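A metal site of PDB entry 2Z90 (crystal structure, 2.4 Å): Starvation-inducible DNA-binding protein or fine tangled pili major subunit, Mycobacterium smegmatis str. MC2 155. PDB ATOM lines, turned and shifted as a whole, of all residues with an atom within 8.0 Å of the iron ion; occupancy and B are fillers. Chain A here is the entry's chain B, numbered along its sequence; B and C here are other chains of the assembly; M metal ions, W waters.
A ring nitrogen (ND1) of His 41 of chain B lies within hydrogen-bond range of the backbone carbonyl oxygen (O) of His 53 of chain B, at 2.6 Å.
A ring nitrogen (NE2) of His 41 of chain B sits close to the side-chain amino group (NZ) of Lys 38 of chain B (3.5 Å).
The indole nitrogen (NE1) of Trp 42 of chain B sits close to the side-chain carboxylate (OD1) of Asp 68, 2.8 Å away.
The side-chain carboxylate (OE2) of Glu 72 lies within salt-bridge range of the side-chain amino group (NZ) of Lys 149 of chain C (3.8 Å).
A ring nitrogen (ND1) of His 41 of chain B lies close to the side-chain carboxylate (OD2) of Asp 57 of chain B (3.4 Å).
The side-chain carboxylate of Asp 68 sits close to the side-chain amino group of Lys 38 of chain B, 2.8 Å away.
The side-chain amino group of Lys 38 of chain B lies within salt-bridge range of the side-chain carboxylate of Asp 57 of chain B.
Lys 38 of chain B touches the iron ion.
OD1 of Asp 57 of chain B touches the iron ion, at 3.7 Å.
Within 4 Å of the iron ion: Asp 68, Glu 72, Lys 38 of chain B, His 41 of chain B and Asp 57 of chain B.
The iron ion is bound by OE1 of Glu 72, 2.1 Å away.
The side-chain carboxylate (OD2) of Asp 68 is bound to the iron ion, 2.3 Å away.
The iron ion is bound by water W1 (2.4 Å).
NE2 of His 41 of chain B binds the iron ion.
The iron ion is bound by OD1 of Asp 68 (2.5 Å).
The iron ion has five donor atoms within binding distance.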
ATOM      1  N   ARG A  64      18.656 -13.974   4.375  1.00  0.00           N
ATOM      2  CA  ARG A  64      17.328 -13.668   3.868  1.00  0.00           C
ATOM      3  C   ARG A  64      17.362 -12.363   3.059  1.00  0.00           C
ATOM      4  O   ARG A  64      16.771 -12.281   1.970  1.00  0.00           O
ATOM      5  CB  ARG A  64      16.343 -13.562   5.018  1.00  0.00           C
ATOM      6  CG  ARG A  64      15.876 -14.912   5.540  1.00  0.00           C
ATOM      7  CD  ARG A  64      15.122 -14.754   6.852  1.00  0.00           C
ATOM      8  NE  ARG A  64      14.429 -15.972   7.268  1.00  0.00           N
ATOM      9  CZ  ARG A  64      13.806 -16.096   8.433  1.00  0.00           C
ATOM     10  NH1 ARG A  64      13.791 -15.082   9.289  1.00  0.00           N
ATOM     11  NH2 ARG A  64      13.178 -17.228   8.742  1.00  0.00           N
ATOM     12  N   GLU A  65      18.037 -11.351   3.601  1.00  0.00           N
ATOM     13  CA  GLU A  65      18.161 -10.068   2.923  1.00  0.00           C
ATOM     14  C   GLU A  65      18.920 -10.255   1.603  1.00  0.00           C
ATOM     15  O   GLU A  65      18.581  -9.630   0.585  1.00  0.00           O
ATOM     16  CB  GLU A  65      18.906  -9.069   3.821  1.00  0.00           C
ATOM     17  CG  GLU A  65      18.050  -8.498   4.948  1.00  0.00           C
ATOM     18  CD  GLU A  65      18.838  -7.666   5.963  1.00  0.00           C
ATOM     19  OE1 GLU A  65      19.644  -6.807   5.534  1.00  0.00           O
ATOM     20  OE2 GLU A  65      18.640  -7.879   7.185  1.00  0.00           O
ATOM     21  N   SER A  67      19.092 -13.053  -0.312  1.00  0.00           N
ATOM     22  CA  SER A  67      18.273 -13.759  -1.292  1.00  0.00           C
ATOM     23  C   SER A  67      17.222 -12.834  -1.879  1.00  0.00           C
ATOM     24  O   SER A  67      16.930 -12.898  -3.083  1.00  0.00           O
ATOM     25  CB  SER A  67      17.631 -15.001  -0.667  1.00  0.00           C
ATOM     26  OG  SER A  67      16.830 -14.674   0.442  1.00  0.00           O
ATOM     27  N   ASP A  68      16.646 -11.952  -1.072  1.00  0.00           N
ATOM     28  CA  ASP A  68      15.641 -11.030  -1.591  1.00  0.00           C
ATOM     29  C   ASP A  68      16.314 -10.022  -2.520  1.00  0.00           C
ATOM     30  O   ASP A  68      15.716  -9.546  -3.480  1.00  0.00           O
ATOM     31  CB  ASP A  68      14.935 -10.293  -0.453  1.00  0.00           C
ATOM     32  CG  ASP A  68      13.771  -9.442  -0.966  1.00  0.00           C
ATOM     33  OD1 ASP A  68      12.777 -10.031  -1.447  1.00  0.00           O
ATOM     34  OD2 ASP A  68      13.867  -8.197  -0.890  1.00  0.00           O
ATOM     35  N   THR A  69      17.566  -9.695  -2.217  1.00  0.00           N
ATOM     36  CA  THR A  69      18.320  -8.751  -3.034  1.00  0.00           C
ATOM     37  C   THR A  69      18.666  -9.370  -4.394  1.00  0.00           C
ATOM     38  O   THR A  69      18.510  -8.727  -5.432  1.00  0.00           O
ATOM     39  CB  THR A  69      19.629  -8.327  -2.336  1.00  0.00           C
ATOM     40  OG1 THR A  69      19.313  -7.483  -1.223  1.00  0.00           O
ATOM     41  CG2 THR A  69      20.558  -7.598  -3.299  1.00  0.00           C
ATOM     42  N   ALA A  71      17.175 -12.079  -5.785  1.00  0.00           N
ATOM     43  CA  ALA A  71      15.941 -12.402  -6.488  1.00  0.00           C
ATOM     44  C   ALA A  71      15.364 -11.181  -7.201  1.00  0.00           C
ATOM     45  O   ALA A  71      14.908 -11.263  -8.349  1.00  0.00           O
ATOM     46  CB  ALA A  71      14.894 -12.971  -5.526  1.00  0.00           C
ATOM     47  N   GLU A  72      15.396 -10.037  -6.515  1.00  0.00           N
ATOM     48  CA  GLU A  72      14.868  -8.822  -7.097  1.00  0.00           C
ATOM     49  C   GLU A  72      15.833  -8.233  -8.120  1.00  0.00           C
ATOM     50  O   GLU A  72      15.411  -7.559  -9.058  1.00  0.00           O
ATOM     51  CB  GLU A  72      14.522  -7.823  -5.983  1.00  0.00           C
ATOM     52  CG  GLU A  72      13.364  -8.346  -5.145  1.00  0.00           C
ATOM     53  CD  GLU A  72      12.915  -7.385  -4.061  1.00  0.00           C
ATOM     54  OE1 GLU A  72      11.891  -7.696  -3.402  1.00  0.00           O
ATOM     55  OE2 GLU A  72      13.567  -6.336  -3.863  1.00  0.00           O
ATOM     56  N   LYS B  38       7.423 -15.468  -0.724  1.00  0.00           N
ATOM     57  CA  LYS B  38       8.514 -14.680  -1.291  1.00  0.00           C
ATOM     58  C   LYS B  38       8.518 -14.878  -2.810  1.00  0.00           C
ATOM     59  O   LYS B  38       8.786 -13.938  -3.564  1.00  0.00           O
ATOM     60  CB  LYS B  38       9.852 -15.112  -0.680  1.00  0.00           C
ATOM     61  CG  LYS B  38      10.743 -13.925  -0.288  1.00  0.00           C
ATOM     62  CD  LYS B  38      10.148 -13.118   0.854  1.00  0.00           C
ATOM     63  CE  LYS B  38      11.064 -11.967   1.265  1.00  0.00           C
ATOM     64  NZ  LYS B  38      10.866 -10.697   0.501  1.00  0.00           N
ATOM     65  N   HIS B  41       5.879 -12.780  -4.086  1.00  0.00           N
ATOM     66  CA  HIS B  41       6.391 -11.433  -3.851  1.00  0.00           C
ATOM     67  C   HIS B  41       7.278 -10.998  -5.013  1.00  0.00           C
ATOM     68  O   HIS B  41       7.183  -9.858  -5.486  1.00  0.00           O
ATOM     69  CB  HIS B  41       7.191 -11.448  -2.539  1.00  0.00           C
ATOM     70  CG  HIS B  41       7.891 -10.159  -2.218  1.00  0.00           C
ATOM     71  ND1 HIS B  41       7.236  -9.042  -1.761  1.00  0.00           N
ATOM     72  CD2 HIS B  41       9.221  -9.847  -2.202  1.00  0.00           C
ATOM     73  CE1 HIS B  41       8.114  -8.090  -1.479  1.00  0.00           C
ATOM     74  NE2 HIS B  41       9.320  -8.561  -1.740  1.00  0.00           N
ATOM     75  N   TRP B  42       8.139 -11.900  -5.487  1.00  0.00           N
ATOM     76  CA  TRP B  42       9.069 -11.581  -6.571  1.00  0.00           C
ATOM     77  C   TRP B  42       8.483 -11.660  -7.979  1.00  0.00           C
ATOM     78  O   TRP B  42       8.782 -10.818  -8.827  1.00  0.00           O
ATOM     79  CB  TRP B  42      10.291 -12.514  -6.549  1.00  0.00           C
ATOM     80  CG  TRP B  42      11.082 -12.540  -5.264  1.00  0.00           C
ATOM     81  CD1 TRP B  42      11.449 -11.470  -4.488  1.00  0.00           C
ATOM     82  CD2 TRP B  42      11.652 -13.693  -4.628  1.00  0.00           C
ATOM     83  NE1 TRP B  42      12.198 -11.880  -3.415  1.00  0.00           N
ATOM     84  CE2 TRP B  42      12.345 -13.242  -3.476  1.00  0.00           C
ATOM     85  CE3 TRP B  42      11.649 -15.065  -4.920  1.00  0.00           C
ATOM     86  CZ2 TRP B  42      13.013 -14.117  -2.612  1.00  0.00           C
ATOM     87  CZ3 TRP B  42      12.320 -15.932  -4.061  1.00  0.00           C
ATOM     88  CH2 TRP B  42      12.992 -15.459  -2.926  1.00  0.00           C
ATOM     89  N   HIS B  53       2.814  -6.840  -3.982  1.00  0.00           N
ATOM     90  CA  HIS B  53       4.231  -7.018  -3.686  1.00  0.00           C
ATOM     91  C   HIS B  53       4.456  -6.777  -2.200  1.00  0.00           C
ATOM     92  O   HIS B  53       5.042  -7.606  -1.506  1.00  0.00           O
ATOM     93  CB  HIS B  53       5.064  -6.039  -4.517  1.00  0.00           C
ATOM     94  CG  HIS B  53       6.545  -6.121  -4.268  1.00  0.00           C
ATOM     95  ND1 HIS B  53       7.307  -7.190  -4.676  1.00  0.00           N
ATOM     96  CD2 HIS B  53       7.398  -5.248  -3.684  1.00  0.00           C
ATOM     97  CE1 HIS B  53       8.573  -6.971  -4.365  1.00  0.00           C
ATOM     98  NE2 HIS B  53       8.649  -5.800  -3.754  1.00  0.00           N
ATOM     99  N   LEU B  54       3.970  -5.637  -1.717  1.00  0.00           N
ATOM    100  CA  LEU B  54       4.116  -5.248  -0.318  1.00  0.00           C
ATOM    101  C   LEU B  54       3.388  -6.145   0.692  1.00  0.00           C
ATOM    102  O   LEU B  54       3.989  -6.596   1.679  1.00  0.00           O
ATOM    103  CB  LEU B  54       3.660  -3.795  -0.119  1.00  0.00           C
ATOM    104  CG  LEU B  54       4.471  -2.691  -0.821  1.00  0.00           C
ATOM    105  CD1 LEU B  54       3.823  -1.332  -0.550  1.00  0.00           C
ATOM    106  CD2 LEU B  54       5.900  -2.713  -0.316  1.00  0.00           C
ATOM    107  N   ASP B  57       5.016  -9.515   1.445  1.00  0.00           N
ATOM    108  CA  ASP B  57       6.152  -9.473   2.358  1.00  0.00           C
ATOM    109  C   ASP B  57       5.644  -9.433   3.796  1.00  0.00           C
ATOM    110  O   ASP B  57       6.247 -10.015   4.696  1.00  0.00           O
ATOM    111  CB  ASP B  57       7.019  -8.233   2.103  1.00  0.00           C
ATOM    112  CG  ASP B  57       8.410  -8.589   1.606  1.00  0.00           C
ATOM    113  OD1 ASP B  57       9.284  -7.683   1.555  1.00  0.00           O
ATOM    114  OD2 ASP B  57       8.638  -9.769   1.250  1.00  0.00           O
ATOM    115  N   LYS C 149      15.804  -1.144 -10.056  1.00  0.00           N
ATOM    116  CA  LYS C 149      14.876  -1.793  -9.141  1.00  0.00           C
ATOM    117  C   LYS C 149      13.594  -0.971  -9.190  1.00  0.00           C
ATOM    118  O   LYS C 149      12.491  -1.511  -9.210  1.00  0.00           O
ATOM    119  CB  LYS C 149      15.434  -1.790  -7.716  1.00  0.00           C
ATOM    120  CG  LYS C 149      14.503  -2.389  -6.665  1.00  0.00           C
ATOM    121  CD  LYS C 149      15.167  -2.343  -5.289  1.00  0.00           C
ATOM    122  CE  LYS C 149      14.239  -2.856  -4.188  1.00  0.00           C
ATOM    123  NZ  LYS C 149      14.900  -2.873  -2.842  1.00  0.00           N
ATOM    124  N   TRP C 152      11.623  -1.571 -12.214  1.00  0.00           N
ATOM    125  CA  TRP C 152      10.893  -2.828 -12.074  1.00  0.00           C
ATOM    126  C   TRP C 152       9.636  -2.635 -11.236  1.00  0.00           C
ATOM    127  O   TRP C 152       8.553  -3.085 -11.608  1.00  0.00           O
ATOM    128  CB  TRP C 152      11.771  -3.902 -11.437  1.00  0.00           C
ATOM    129  CG  TRP C 152      10.991  -5.068 -10.876  1.00  0.00           C
ATOM    130  CD1 TRP C 152      10.069  -5.842 -11.541  1.00  0.00           C
ATOM    131  CD2 TRP C 152      11.044  -5.586  -9.540  1.00  0.00           C
ATOM    132  NE1 TRP C 152       9.550  -6.807 -10.693  1.00  0.00           N
ATOM    133  CE2 TRP C 152      10.135  -6.668  -9.464  1.00  0.00           C
ATOM    134  CE3 TRP C 152      11.776  -5.248  -8.395  1.00  0.00           C
ATOM    135  CZ2 TRP C 152       9.945  -7.413  -8.295  1.00  0.00           C
ATOM    136  CZ3 TRP C 152      11.589  -5.985  -7.230  1.00  0.00           C
ATOM    137  CH2 TRP C 152      10.673  -7.049  -7.191  1.00  0.00           C
ATOM    138  N   LEU C 153       9.772  -1.961 -10.112  1.00  0.00           N
ATOM    139  CA  LEU C 153       8.629  -1.742  -9.235  1.00  0.00           C
ATOM    140  C   LEU C 153       7.497  -0.977  -9.909  1.00  0.00           C
ATOM    141  O   LEU C 153       6.330  -1.243  -9.663  1.00  0.00           O
ATOM    142  CB  LEU C 153       9.078  -1.055  -7.944  1.00  0.00           C
ATOM    143  CG  LEU C 153      10.139  -1.817  -7.135  1.00  0.00           C
ATOM    144  CD1 LEU C 153      10.609  -0.956  -5.971  1.00  0.00           C
ATOM    145  CD2 LEU C 153       9.558  -3.156  -6.625  1.00  0.00           C
HETATM  146 FE    FE M   1      11.602  -7.868  -1.368  1.00  0.00          FE
HETATM  147  O   HOH W   1      11.577  -5.483  -1.184  1.00  0.00           O
